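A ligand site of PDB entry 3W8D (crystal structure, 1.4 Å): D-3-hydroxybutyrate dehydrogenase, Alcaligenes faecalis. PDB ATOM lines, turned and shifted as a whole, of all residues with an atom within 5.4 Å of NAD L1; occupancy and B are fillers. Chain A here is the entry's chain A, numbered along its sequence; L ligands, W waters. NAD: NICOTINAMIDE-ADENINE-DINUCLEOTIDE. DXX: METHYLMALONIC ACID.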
ATOM      1  N   GLY A  11       9.617 -11.374  -6.652  1.00  0.00           N
ATOM      2  CA  GLY A  11      10.412 -10.249  -6.135  1.00  0.00           C
ATOM      3  C   GLY A  11      11.294 -10.692  -5.020  1.00  0.00           C
ATOM      4  O   GLY A  11      11.405  -9.991  -3.990  1.00  0.00           O
ATOM      5  N   SER A  12      12.070 -11.784  -5.280  1.00  0.00           N
ATOM      6  CA  SER A  12      12.967 -12.363  -4.223  1.00  0.00           C
ATOM      7  C   SER A  12      14.446 -12.094  -4.567  1.00  0.00           C
ATOM      8  O   SER A  12      15.305 -12.746  -3.965  1.00  0.00           O
ATOM      9  CB  SER A  12      12.673 -13.797  -4.041  1.00  0.00           C
ATOM     10  OG  SER A  12      12.507 -14.463  -5.328  1.00  0.00           O
ATOM     11  N   THR A  13      14.698 -11.102  -5.386  1.00  0.00           N
ATOM     12  CA  THR A  13      16.139 -10.718  -5.658  1.00  0.00           C
ATOM     13  C   THR A  13      16.585  -9.612  -4.688  1.00  0.00           C
ATOM     14  O   THR A  13      17.784  -9.199  -4.756  1.00  0.00           O
ATOM     15  CB  THR A  13      16.284 -10.279  -7.136  1.00  0.00           C
ATOM     16  OG1 THR A  13      15.339  -9.221  -7.390  1.00  0.00           O
ATOM     17  CG2 THR A  13      16.072 -11.479  -8.091  1.00  0.00           C
ATOM     18  N   SER A  14      15.747  -9.133  -3.796  1.00  0.00           N
ATOM     19  CA  SER A  14      16.111  -8.048  -2.866  1.00  0.00           C
ATOM     20  C   SER A  14      15.235  -8.151  -1.674  1.00  0.00           C
ATOM     21  O   SER A  14      14.129  -8.734  -1.730  1.00  0.00           O
ATOM     22  CB  SER A  14      15.812  -6.658  -3.597  1.00  0.00           C
ATOM     23  OG  SER A  14      16.008  -5.532  -2.744  1.00  0.00           O
ATOM     24  N   GLY A  15      15.661  -7.524  -0.578  1.00  0.00           N
ATOM     25  CA  GLY A  15      14.691  -7.149   0.451  1.00  0.00           C
ATOM     26  C   GLY A  15      14.007  -8.305   1.109  1.00  0.00           C
ATOM     27  O   GLY A  15      14.595  -9.363   1.487  1.00  0.00           O
ATOM     28  N   ILE A  16      12.709  -8.083   1.385  1.00  0.00           N
ATOM     29  CA  ILE A  16      11.947  -9.075   2.098  1.00  0.00           C
ATOM     30  C   ILE A  16      11.866 -10.383   1.340  1.00  0.00           C
ATOM     31  O   ILE A  16      11.922 -11.472   1.944  1.00  0.00           O
ATOM     32  CB  ILE A  16      10.529  -8.455   2.374  1.00  0.00           C
ATOM     33  CG1 ILE A  16      10.663  -7.290   3.360  1.00  0.00           C
ATOM     34  CG2 ILE A  16       9.559  -9.541   2.889  1.00  0.00           C
ATOM     35  CD1 ILE A  16       9.351  -6.378   3.332  1.00  0.00           C
ATOM     36  N   GLY A  17      11.610 -10.319   0.032  1.00  0.00           N
ATOM     37  CA  GLY A  17      11.519 -11.546  -0.732  1.00  0.00           C
ATOM     38  C   GLY A  17      12.769 -12.377  -0.753  1.00  0.00           C
ATOM     39  O   GLY A  17      12.677 -13.604  -0.748  1.00  0.00           O
ATOM     40  N   ASN A  34      12.815 -14.714  -8.360  1.00  0.00           N
ATOM     41  CA  ASN A  34      12.223 -13.894  -9.423  1.00  0.00           C
ATOM     42  C   ASN A  34      12.543 -12.460  -9.096  1.00  0.00           C
ATOM     43  O   ASN A  34      12.716 -12.119  -7.902  1.00  0.00           O
ATOM     44  CB  ASN A  34      10.689 -14.123  -9.428  1.00  0.00           C
ATOM     45  CG  ASN A  34       9.954 -13.048 -10.157  1.00  0.00           C
ATOM     46  OD1 ASN A  34       9.391 -12.144  -9.512  1.00  0.00           O
ATOM     47  ND2 ASN A  34       9.931 -13.084 -11.491  1.00  0.00           N
ATOM     48  N   GLY A  35      12.639 -11.533 -10.078  1.00  0.00           N
ATOM     49  CA  GLY A  35      12.876 -10.138  -9.833  1.00  0.00           C
ATOM     50  C   GLY A  35      13.988  -9.600 -10.653  1.00  0.00           C
ATOM     51  O   GLY A  35      14.673 -10.303 -11.400  1.00  0.00           O
ATOM     52  N   PHE A  36      14.200  -8.332 -10.464  1.00  0.00           N
ATOM     53  CA  PHE A  36      15.197  -7.629 -11.247  1.00  0.00           C
ATOM     54  C   PHE A  36      16.457  -7.570 -10.432  1.00  0.00           C
ATOM     55  O   PHE A  36      16.527  -7.793  -9.240  1.00  0.00           O
ATOM     56  CB  PHE A  36      14.695  -6.220 -11.581  1.00  0.00           C
ATOM     57  CG  PHE A  36      13.438  -6.251 -12.362  1.00  0.00           C
ATOM     58  CD1 PHE A  36      12.367  -5.385 -12.010  1.00  0.00           C
ATOM     59  CD2 PHE A  36      13.240  -7.187 -13.357  1.00  0.00           C
ATOM     60  CE1 PHE A  36      11.222  -5.396 -12.744  1.00  0.00           C
ATOM     61  CE2 PHE A  36      11.981  -7.262 -14.080  1.00  0.00           C
ATOM     62  CZ  PHE A  36      11.013  -6.299 -13.780  1.00  0.00           C
ATOM     63  N   GLY A  37      17.560  -7.161 -11.119  1.00  0.00           N
ATOM     64  CA  GLY A  37      18.861  -6.863 -10.412  1.00  0.00           C
ATOM     65  C   GLY A  37      20.002  -7.229 -11.340  1.00  0.00           C
ATOM     66  O   GLY A  37      19.836  -7.612 -12.514  1.00  0.00           O
ATOM     67  N   ALA A  62      10.531 -12.595 -14.825  1.00  0.00           N
ATOM     68  CA  ALA A  62       9.207 -12.240 -15.389  1.00  0.00           C
ATOM     69  C   ALA A  62       8.913 -10.881 -14.836  1.00  0.00           C
ATOM     70  O   ALA A  62       9.081 -10.612 -13.617  1.00  0.00           O
ATOM     71  CB  ALA A  62       8.174 -13.235 -14.923  1.00  0.00           C
ATOM     72  N   ASP A  63       8.412  -9.952 -15.676  1.00  0.00           N
ATOM     73  CA  ASP A  63       7.894  -8.704 -15.213  1.00  0.00           C
ATOM     74  C   ASP A  63       6.439  -8.921 -14.891  1.00  0.00           C
ATOM     75  O   ASP A  63       5.546  -9.085 -15.773  1.00  0.00           O
ATOM     76  CB  ASP A  63       8.038  -7.637 -16.328  1.00  0.00           C
ATOM     77  CG  ASP A  63       7.485  -6.296 -15.938  1.00  0.00           C
ATOM     78  OD1 ASP A  63       7.731  -5.309 -16.687  1.00  0.00           O
ATOM     79  OD2 ASP A  63       6.765  -6.120 -14.959  1.00  0.00           O
ATOM     80  N   LEU A  64       6.111  -8.914 -13.587  1.00  0.00           N
ATOM     81  CA  LEU A  64       4.795  -9.355 -13.136  1.00  0.00           C
ATOM     82  C   LEU A  64       3.770  -8.246 -13.271  1.00  0.00           C
ATOM     83  O   LEU A  64       2.636  -8.465 -12.917  1.00  0.00           O
ATOM     84  CB  LEU A  64       4.936  -9.822 -11.698  1.00  0.00           C
ATOM     85  CG  LEU A  64       5.864 -11.043 -11.583  1.00  0.00           C
ATOM     86  CD1 LEU A  64       5.998 -11.455 -10.071  1.00  0.00           C
ATOM     87  CD2 LEU A  64       5.530 -12.285 -12.404  1.00  0.00           C
ATOM     88  N   SER A  65       4.170  -7.070 -13.765  1.00  0.00           N
ATOM     89  CA  SER A  65       3.149  -6.104 -14.176  1.00  0.00           C
ATOM     90  C   SER A  65       2.331  -6.533 -15.410  1.00  0.00           C
ATOM     91  O   SER A  65       1.263  -5.979 -15.675  1.00  0.00           O
ATOM     92  CB  SER A  65       3.737  -4.726 -14.429  1.00  0.00           C
ATOM     93  OG  SER A  65       4.527  -4.747 -15.597  1.00  0.00           O
ATOM     94  N   ASN A  90       5.064 -11.430  -3.291  1.00  0.00           N
ATOM     95  CA  ASN A  90       5.819 -10.418  -2.586  1.00  0.00           C
ATOM     96  C   ASN A  90       6.246  -9.212  -3.381  1.00  0.00           C
ATOM     97  O   ASN A  90       6.344  -8.101  -2.818  1.00  0.00           O
ATOM     98  CB  ASN A  90       7.109 -11.090  -1.939  1.00  0.00           C
ATOM     99  CG  ASN A  90       8.088 -10.114  -1.494  1.00  0.00           C
ATOM    100  OD1 ASN A  90       7.998  -9.578  -0.336  1.00  0.00           O
ATOM    101  ND2 ASN A  90       9.071  -9.830  -2.319  1.00  0.00           N
ATOM    102  N   ALA A  91       6.480  -9.371  -4.706  1.00  0.00           N
ATOM    103  CA  ALA A  91       7.032  -8.244  -5.457  1.00  0.00           C
ATOM    104  C   ALA A  91       6.201  -6.965  -5.330  1.00  0.00           C
ATOM    105  O   ALA A  91       4.907  -7.082  -5.406  1.00  0.00           O
ATOM    106  CB  ALA A  91       7.100  -8.640  -6.939  1.00  0.00           C
ATOM    107  N   GLY A  92       6.741  -5.787  -5.135  1.00  0.00           N
ATOM    108  CA  GLY A  92       5.919  -4.604  -5.084  1.00  0.00           C
ATOM    109  C   GLY A  92       6.824  -3.416  -5.186  1.00  0.00           C
ATOM    110  O   GLY A  92       8.049  -3.543  -4.927  1.00  0.00           O
ATOM    111  N   ILE A  93       6.212  -2.274  -5.471  1.00  0.00           N
ATOM    112  CA  ILE A  93       6.898  -0.981  -5.604  1.00  0.00           C
ATOM    113  C   ILE A  93       6.138   0.112  -4.878  1.00  0.00           C
ATOM    114  O   ILE A  93       4.921  -0.029  -4.527  1.00  0.00           O
ATOM    115  CB  ILE A  93       7.070  -0.580  -7.110  1.00  0.00           C
ATOM    116  CG1 ILE A  93       5.677  -0.649  -7.832  1.00  0.00           C
ATOM    117  CG2 ILE A  93       8.098  -1.563  -7.850  1.00  0.00           C
ATOM    118  CD1 ILE A  93       5.778   0.023  -9.222  1.00  0.00           C
ATOM    119  N   LEU A 113       1.368  -4.284 -10.383  1.00  0.00           N
ATOM    120  CA  LEU A 113       2.266  -5.181  -9.707  1.00  0.00           C
ATOM    121  C   LEU A 113       1.744  -5.524  -8.339  1.00  0.00           C
ATOM    122  O   LEU A 113       1.693  -6.674  -7.938  1.00  0.00           O
ATOM    123  CB  LEU A 113       3.685  -4.521  -9.595  1.00  0.00           C
ATOM    124  CG  LEU A 113       4.682  -5.438  -8.857  1.00  0.00           C
ATOM    125  CD1 LEU A 113       4.929  -6.730  -9.704  1.00  0.00           C
ATOM    126  CD2 LEU A 113       5.966  -4.718  -8.649  1.00  0.00           C
ATOM    127  N   ASN A 114       1.445  -4.480  -7.562  1.00  0.00           N
ATOM    128  CA  ASN A 114       1.119  -4.699  -6.161  1.00  0.00           C
ATOM    129  C   ASN A 114      -0.257  -5.318  -5.932  1.00  0.00           C
ATOM    130  O   ASN A 114      -0.482  -5.952  -4.897  1.00  0.00           O
ATOM    131  CB  ASN A 114       1.166  -3.426  -5.342  1.00  0.00           C
ATOM    132  CG  ASN A 114       2.525  -2.778  -5.234  1.00  0.00           C
ATOM    133  OD1 ASN A 114       3.403  -3.039  -6.050  1.00  0.00           O
ATOM    134  ND2 ASN A 114       2.686  -1.879  -4.302  1.00  0.00           N
ATOM    135  N   ILE A 140       2.138 -10.606   0.604  1.00  0.00           N
ATOM    136  CA  ILE A 140       2.826  -9.570   1.378  1.00  0.00           C
ATOM    137  C   ILE A 140       2.088  -8.273   1.096  1.00  0.00           C
ATOM    138  O   ILE A 140       2.240  -7.659   0.022  1.00  0.00           O
ATOM    139  CB  ILE A 140       4.300  -9.441   1.023  1.00  0.00           C
ATOM    140  CG1 ILE A 140       5.069 -10.766   1.125  1.00  0.00           C
ATOM    141  CG2 ILE A 140       4.943  -8.462   2.040  1.00  0.00           C
ATOM    142  CD1 ILE A 140       4.859 -11.627   2.425  1.00  0.00           C
ATOM    143  N   ALA A 141       1.216  -7.900   2.054  1.00  0.00           N
ATOM    144  CA  ALA A 141       0.475  -6.668   2.014  1.00  0.00           C
ATOM    145  C   ALA A 141       1.279  -5.602   2.682  1.00  0.00           C
ATOM    146  O   ALA A 141       2.447  -5.368   2.265  1.00  0.00           O
ATOM    147  CB  ALA A 141      -0.989  -6.846   2.511  1.00  0.00           C
ATOM    148  N   SER A 142       0.794  -4.984   3.767  1.00  0.00           N
ATOM    149  CA  SER A 142       1.525  -3.903   4.482  1.00  0.00           C
ATOM    150  C   SER A 142       0.615  -3.441   5.602  1.00  0.00           C
ATOM    151  O   SER A 142      -0.646  -3.730   5.573  1.00  0.00           O
ATOM    152  CB  SER A 142       1.721  -2.684   3.533  1.00  0.00           C
ATOM    153  OG  SER A 142       2.239  -1.602   4.281  1.00  0.00           O
ATOM    154  N   ALA A 143       1.163  -2.765   6.607  1.00  0.00           N
ATOM    155  CA  ALA A 143       0.287  -1.965   7.461  1.00  0.00           C
ATOM    156  C   ALA A 143      -0.656  -1.090   6.630  1.00  0.00           C
ATOM    157  O   ALA A 143      -1.790  -0.831   7.038  1.00  0.00           O
ATOM    158  CB  ALA A 143       1.208  -1.072   8.391  1.00  0.00           C
ATOM    159  N   TYR A 155      -0.512   3.000  -3.473  1.00  0.00           N
ATOM    160  CA  TYR A 155      -0.007   1.886  -2.727  1.00  0.00           C
ATOM    161  C   TYR A 155      -1.030   1.413  -1.626  1.00  0.00           C
ATOM    162  O   TYR A 155      -1.246   0.194  -1.483  1.00  0.00           O
ATOM    163  CB  TYR A 155       1.292   2.357  -2.070  1.00  0.00           C
ATOM    164  CG  TYR A 155       2.031   1.268  -1.269  1.00  0.00           C
ATOM    165  CD1 TYR A 155       1.814   1.084   0.097  1.00  0.00           C
ATOM    166  CD2 TYR A 155       2.982   0.456  -1.912  1.00  0.00           C
ATOM    167  CE1 TYR A 155       2.538   0.062   0.776  1.00  0.00           C
ATOM    168  CE2 TYR A 155       3.741  -0.473  -1.260  1.00  0.00           C
ATOM    169  CZ  TYR A 155       3.522  -0.654   0.076  1.00  0.00           C
ATOM    170  OH  TYR A 155       4.201  -1.636   0.726  1.00  0.00           O
ATOM    171  N   LYS A 159      -2.700  -2.175  -1.538  1.00  0.00           N
ATOM    172  CA  LYS A 159      -2.502  -3.082  -0.405  1.00  0.00           C
ATOM    173  C   LYS A 159      -3.815  -3.418   0.291  1.00  0.00           C
ATOM    174  O   LYS A 159      -3.991  -4.555   0.746  1.00  0.00           O
ATOM    175  CB  LYS A 159      -1.466  -2.469   0.582  1.00  0.00           C
ATOM    176  CG  LYS A 159      -0.045  -2.428   0.014  1.00  0.00           C
ATOM    177  CD  LYS A 159       0.490  -3.817  -0.424  1.00  0.00           C
ATOM    178  CE  LYS A 159       2.059  -3.763  -0.650  1.00  0.00           C
ATOM    179  NZ  LYS A 159       2.594  -5.037  -1.008  1.00  0.00           N
ATOM    180  N   PRO A 185       3.600  -5.971   7.008  1.00  0.00           N
ATOM    181  CA  PRO A 185       4.744  -5.357   7.702  1.00  0.00           C
ATOM    182  C   PRO A 185       4.549  -3.882   7.905  1.00  0.00           C
ATOM    183  O   PRO A 185       3.932  -3.189   7.094  1.00  0.00           O
ATOM    184  CB  PRO A 185       6.005  -5.589   6.779  1.00  0.00           C
ATOM    185  CG  PRO A 185       5.538  -6.716   5.813  1.00  0.00           C
ATOM    186  CD  PRO A 185       4.014  -6.402   5.633  1.00  0.00           C
ATOM    187  N   GLY A 186       5.152  -3.454   9.048  1.00  0.00           N
ATOM    188  CA  GLY A 186       5.484  -2.038   9.192  1.00  0.00           C
ATOM    189  C   GLY A 186       6.795  -1.750   8.462  1.00  0.00           C
ATOM    190  O   GLY A 186       7.186  -2.451   7.525  1.00  0.00           O
ATOM    191  N   TRP A 187       7.489  -0.682   8.890  1.00  0.00           N
ATOM    192  CA  TRP A 187       8.761  -0.357   8.195  1.00  0.00           C
ATOM    193  C   TRP A 187       9.825  -1.415   8.331  1.00  0.00           C
ATOM    194  O   TRP A 187      10.063  -1.928   9.439  1.00  0.00           O
ATOM    195  CB  TRP A 187       9.411   0.926   8.844  1.00  0.00           C
ATOM    196  CG  TRP A 187       8.689   2.194   8.717  1.00  0.00           C
ATOM    197  CD1 TRP A 187       8.123   2.903   9.749  1.00  0.00           C
ATOM    198  CD2 TRP A 187       8.424   2.942   7.528  1.00  0.00           C
ATOM    199  NE1 TRP A 187       7.619   4.121   9.257  1.00  0.00           N
ATOM    200  CE2 TRP A 187       7.771   4.130   7.915  1.00  0.00           C
ATOM    201  CE3 TRP A 187       8.743   2.776   6.191  1.00  0.00           C
ATOM    202  CZ2 TRP A 187       7.339   5.109   6.950  1.00  0.00           C
ATOM    203  CZ3 TRP A 187       8.394   3.745   5.265  1.00  0.00           C
ATOM    204  CH2 TRP A 187       7.750   4.883   5.661  1.00  0.00           C
ATOM    205  N   VAL A 188      10.448  -1.765   7.205  1.00  0.00           N
ATOM    206  CA  VAL A 188      11.527  -2.774   7.050  1.00  0.00           C
ATOM    207  C   VAL A 188      12.573  -2.017   6.231  1.00  0.00           C
ATOM    208  O   VAL A 188      12.248  -1.420   5.181  1.00  0.00           O
ATOM    209  CB  VAL A 188      11.035  -3.971   6.238  1.00  0.00           C
ATOM    210  CG1 VAL A 188      12.140  -5.010   6.107  1.00  0.00           C
ATOM    211  CG2 VAL A 188       9.788  -4.604   6.896  1.00  0.00           C
ATOM    212  N   ARG A 189      13.846  -2.024   6.674  1.00  0.00           N
ATOM    213  CA  ARG A 189      14.836  -1.169   6.003  1.00  0.00           C
ATOM    214  C   ARG A 189      15.399  -1.854   4.757  1.00  0.00           C
ATOM    215  O   ARG A 189      16.554  -2.259   4.765  1.00  0.00           O
ATOM    216  CB  ARG A 189      15.958  -0.852   6.949  1.00  0.00           C
ATOM    217  CG  ARG A 189      16.570   0.482   6.462  1.00  0.00           C
ATOM    218  CD  ARG A 189      17.644   0.974   7.470  1.00  0.00           C
ATOM    219  NE  ARG A 189      18.227   2.229   6.930  1.00  0.00           N
ATOM    220  CZ  ARG A 189      18.920   3.096   7.693  1.00  0.00           C
ATOM    221  NH1 ARG A 189      19.086   2.898   9.002  1.00  0.00           N
ATOM    222  NH2 ARG A 189      19.441   4.163   7.085  1.00  0.00           N
ATOM    223  N   THR A 190      14.653  -1.819   3.665  1.00  0.00           N
ATOM    224  CA  THR A 190      15.034  -2.315   2.349  1.00  0.00           C
ATOM    225  C   THR A 190      15.164  -1.060   1.418  1.00  0.00           C
ATOM    226  O   THR A 190      14.890   0.110   1.808  1.00  0.00           O
ATOM    227  CB  THR A 190      13.905  -3.165   1.745  1.00  0.00           C
ATOM    228  OG1 THR A 190      12.821  -2.261   1.480  1.00  0.00           O
ATOM    229  CG2 THR A 190      13.361  -4.257   2.727  1.00  0.00           C
ATOM    230  N   PRO A 191      15.585  -1.306   0.130  1.00  0.00           N
ATOM    231  CA  PRO A 191      15.668  -0.084  -0.773  1.00  0.00           C
ATOM    232  C   PRO A 191      14.402   0.702  -0.995  1.00  0.00           C
ATOM    233  O   PRO A 191      14.438   1.909  -1.200  1.00  0.00           O
ATOM    234  CB  PRO A 191      16.193  -0.666  -2.082  1.00  0.00           C
ATOM    235  CG  PRO A 191      16.936  -1.990  -1.688  1.00  0.00           C
ATOM    236  CD  PRO A 191      16.112  -2.545  -0.464  1.00  0.00           C
ATOM    237  N   LEU A 192      13.250   0.014  -0.843  1.00  0.00           N
ATOM    238  CA  LEU A 192      11.973   0.685  -1.004  1.00  0.00           C
ATOM    239  C   LEU A 192      11.807   1.785   0.085  1.00  0.00           C
ATOM    240  O   LEU A 192      11.188   2.813  -0.159  1.00  0.00           O
ATOM    241  CB  LEU A 192      10.865  -0.408  -0.921  1.00  0.00           C
ATOM    242  CG  LEU A 192       9.375   0.084  -1.040  1.00  0.00           C
ATOM    243  CD1 LEU A 192       8.654  -1.056  -1.613  1.00  0.00           C
ATOM    244  CD2 LEU A 192       8.735   0.555   0.379  1.00  0.00           C
ATOM    245  N   VAL A 193      12.342   1.554   1.310  1.00  0.00           N
ATOM    246  CA  VAL A 193      12.269   2.462   2.457  1.00  0.00           C
ATOM    247  C   VAL A 193      13.468   3.403   2.436  1.00  0.00           C
ATOM    248  O   VAL A 193      13.332   4.526   2.854  1.00  0.00           O
ATOM    249  CB  VAL A 193      12.125   1.635   3.734  1.00  0.00           C
ATOM    250  CG1 VAL A 193      12.392   2.424   5.022  1.00  0.00           C
ATOM    251  CG2 VAL A 193      10.680   1.017   3.732  1.00  0.00           C
HETATM  252  PA  NAD L   1      12.553  -4.192  -2.540  1.00  0.00           P
HETATM  253  O1A NAD L   1      12.507  -3.045  -3.416  1.00  0.00           O
HETATM  254  O2A NAD L   1      13.790  -4.292  -1.752  1.00  0.00           O
HETATM  255  O5B NAD L   1      12.250  -5.513  -3.360  1.00  0.00           O
HETATM  256  C5B NAD L   1      11.229  -5.499  -4.413  1.00  0.00           C
HETATM  257  C4B NAD L   1      11.427  -6.854  -5.090  1.00  0.00           C
HETATM  258  O4B NAD L   1      10.409  -6.859  -6.155  1.00  0.00           O
HETATM  259  C3B NAD L   1      12.757  -6.872  -5.879  1.00  0.00           C
HETATM  260  O3B NAD L   1      13.168  -8.224  -6.004  1.00  0.00           O
HETATM  261  C2B NAD L   1      12.381  -6.297  -7.240  1.00  0.00           C
HETATM  262  O2B NAD L   1      13.307  -6.682  -8.300  1.00  0.00           O
HETATM  263  C1B NAD L   1      11.041  -6.956  -7.478  1.00  0.00           C
HETATM  264  N9A NAD L   1      10.237  -6.377  -8.493  1.00  0.00           N
HETATM  265  C8A NAD L   1      10.003  -5.008  -8.697  1.00  0.00           C
HETATM  266  N7A NAD L   1       9.252  -4.803  -9.779  1.00  0.00           N
HETATM  267  C5A NAD L   1       8.948  -6.064 -10.285  1.00  0.00           C
HETATM  268  C6A NAD L   1       8.246  -6.538 -11.393  1.00  0.00           C
HETATM  269  N6A NAD L   1       7.562  -5.684 -12.239  1.00  0.00           N
HETATM  270  N1A NAD L   1       8.193  -7.893 -11.552  1.00  0.00           N
HETATM  271  C2A NAD L   1       8.838  -8.744 -10.766  1.00  0.00           C
HETATM  272  N3A NAD L   1       9.581  -8.377  -9.688  1.00  0.00           N
HETATM  273  C4A NAD L   1       9.550  -7.038  -9.477  1.00  0.00           C
HETATM  274  O3  NAD L   1      11.273  -3.982  -1.583  1.00  0.00           O
HETATM  275  PN  NAD L   1      10.738  -4.684  -0.263  1.00  0.00           P
HETATM  276  O1N NAD L   1      10.674  -3.626   0.742  1.00  0.00           O
HETATM  277  O2N NAD L   1      11.432  -5.913   0.024  1.00  0.00           O
HETATM  278  O5D NAD L   1       9.260  -5.032  -0.727  1.00  0.00           O
HETATM  279  C5D NAD L   1       8.737  -6.385  -0.848  1.00  0.00           C
HETATM  280  C4D NAD L   1       7.273  -6.313  -0.508  1.00  0.00           C
HETATM  281  O4D NAD L   1       7.088  -5.906   0.898  1.00  0.00           O
HETATM  282  C3D NAD L   1       6.509  -5.337  -1.414  1.00  0.00           C
HETATM  283  O3D NAD L   1       5.199  -5.940  -1.744  1.00  0.00           O
HETATM  284  C2D NAD L   1       6.250  -4.150  -0.506  1.00  0.00           C
HETATM  285  O2D NAD L   1       5.059  -3.463  -0.872  1.00  0.00           O
HETATM  286  C1D NAD L   1       6.108  -4.871   0.840  1.00  0.00           C
HETATM  287  N1N NAD L   1       6.258  -4.050   2.052  1.00  0.00           N
HETATM  288  C2N NAD L   1       7.493  -3.488   2.352  1.00  0.00           C
HETATM  289  C3N NAD L   1       7.651  -2.743   3.489  1.00  0.00           C
HETATM  290  C7N NAD L   1       8.919  -2.094   3.863  1.00  0.00           C
HETATM  291  O7N NAD L   1       8.910  -1.306   4.873  1.00  0.00           O
HETATM  292  N7N NAD L   1      10.034  -2.377   3.182  1.00  0.00           N
HETATM  293  C4N NAD L   1       6.589  -2.593   4.399  1.00  0.00           C
HETATM  294  C5N NAD L   1       5.327  -3.226   4.088  1.00  0.00           C
HETATM  295  C6N NAD L   1       5.157  -3.999   2.916  1.00  0.00           C
HETATM  296  C1  DXX L   2       5.228   0.143   3.233  1.00  0.00           C
HETATM  297  O1  DXX L   2       3.994   0.056   3.522  1.00  0.00           O
HETATM  298  OXT DXX L   2       5.703  -0.493   2.279  1.00  0.00           O
HETATM  299  CA  DXX L   2       6.144   1.102   3.910  1.00  0.00           C
HETATM  300  CB  DXX L   2       5.775   1.145   5.432  1.00  0.00           C
HETATM  301  C   DXX L   2       5.802   2.369   3.201  1.00  0.00           C
HETATM  302  O   DXX L   2       6.459   2.715   2.183  1.00  0.00           O
HETATM  303  O2  DXX L   2       4.881   3.075   3.628  1.00  0.00           O
HETATM  304  O   HOH W   1      14.462  -3.425  -5.794  1.00  0.00           O
HETATM  305  O   HOH W   2      13.462  -0.055  -4.099  1.00  0.00           O
HETATM  306  O   HOH W   3      15.030  -4.743  -8.132  1.00  0.00           O
HETATM  307  O   HOH W   4      11.747  -2.690  -7.213  1.00  0.00           O
HETATM  308  O   HOH W   5      10.397  -1.952  -4.816  1.00  0.00           O
HETATM  309  O   HOH W   6      11.360  -8.062  -1.696  1.00  0.00           O
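Water W5 lies within hydrogen-bond range of an oxygen (O1A) of NAD L1 and the backbone carbonyl oxygen of Gly 92.
Water W2 lies within hydrogen-bond range of an oxygen (O1A) of NAD L1 (3.2 Å) and the backbone NH (N) of Leu 192 (3.3 Å).
O of Gly 11 lies within hydrogen-bond range of O3B of NAD L1 (3.2 Å).
The backbone NH of Ile 16 lies within hydrogen-bond range of an oxygen (O2N) of NAD L1, at 2.9 Å.
The backbone NH (N) of Phe 36 lies within hydrogen-bond range of an oxygen (O2B) of NAD L1 (2.9 Å).
An oxygen (O3D) of NAD L1 lies within hydrogen-bond range of the backbone carbonyl oxygen (O) of Asn 90, 2.7 Å away.
A nitrogen (N6A) of NAD L1 is in hydrogen-bond range of the side-chain carboxylate of Asp 63 (2.9 Å).
The side-chain hydroxyl (OG) of Ser 142 lies within hydrogen-bond range of an oxygen (O1) of DXX L2 (2.5 Å).
The side-chain hydroxyl (OG1) of Thr 13 is in hydrogen-bond range of an oxygen (O3B) of NAD L1.
The side-chain hydroxyl of Tyr 155 lies within hydrogen-bond range of an oxygen (OXT) of DXX L2, at 2.4 Å.
An oxygen (O3B) of NAD L1 lies within hydrogen-bond range of the backbone NH of Thr 13, 3.3 Å away.
The backbone NH (N) of Val 188 sits at hydrogen-bond distance from an oxygen (O7N) of NAD L1 (2.8 Å).
O of Val 188 is in hydrogen-bond range of N7N of NAD L1.
The side-chain amino group (NZ) of Lys 159 is in hydrogen-bond range of an oxygen (O3D) of NAD L1 (2.9 Å).
The side-chain hydroxyl (OH) of Tyr 155 sits at hydrogen-bond distance from an oxygen (O2D) of NAD L1 (2.6 Å).
N of Leu 64 lies within hydrogen-bond range of N1A of NAD L1 (3.1 Å).
OG of Ser 14 sits at hydrogen-bond distance from O2A of NAD L1, at 2.7 Å.
The side-chain hydroxyl of Thr 190 is in hydrogen-bond range of an oxygen (O1N) of NAD L1, 2.6 Å away.
The backbone carbonyl oxygen (O) of Ile 93 is in hydrogen-bond range of the side-chain amide nitrogen (ND2) of Asn 114 (2.9 Å).
The backbone NH (N) of Ser 12 sits at hydrogen-bond distance from the backbone carbonyl oxygen (O) of Asn 34, at 2.7 Å.
ND2 of Asn 90 sits at hydrogen-bond distance from O of Gly 11 (2.9 Å).
The backbone carbonyl oxygen (O) of Ala 62 sits at hydrogen-bond distance from the side-chain amide nitrogen (ND2) of Asn 34 (3.4 Å).
The side-chain carboxylate of Asp 63 lies within hydrogen-bond range of the side-chain hydroxyl of Ser 65, at 2.7 Å.
The side-chain amino group of Lys 159 sits at hydrogen-bond distance from the backbone carbonyl oxygen of Ala 141 (3.3 Å).
The backbone NH (N) of Leu 192 lies close to the side-chain hydroxyl (OG1) of Thr 190.
The backbone carbonyl oxygen (O) of Pro 185 lies within hydrogen-bond range of the backbone NH (N) of Ala 143, 2.8 Å away.
O of Gly 186 lies close to O7N of NAD L1, 3.4 Å away.
Residues that only touch NAD L1: Ser 12 (3.8 Å), Gly 15 (3.5 Å), Asn 34 (3.7 Å), Gly 35 (3.7 Å), Ala 62 (3.4 Å), Ser 65 (3.97 Å), Ala 91 (3.7 Å), Gly 92 (3.7 Å), Ile 93 (3.9 Å), Leu 113 (3.5 Å), Ile 140 (3.5 Å), Ala 141 (3.1 Å), Ser 142 (3.5 Å), Pro 185 (3.3 Å), Trp 187 (3.5 Å), Pro 191 (3.2 Å), Leu 192 (3.6 Å) and Val 193 (3.1 Å).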
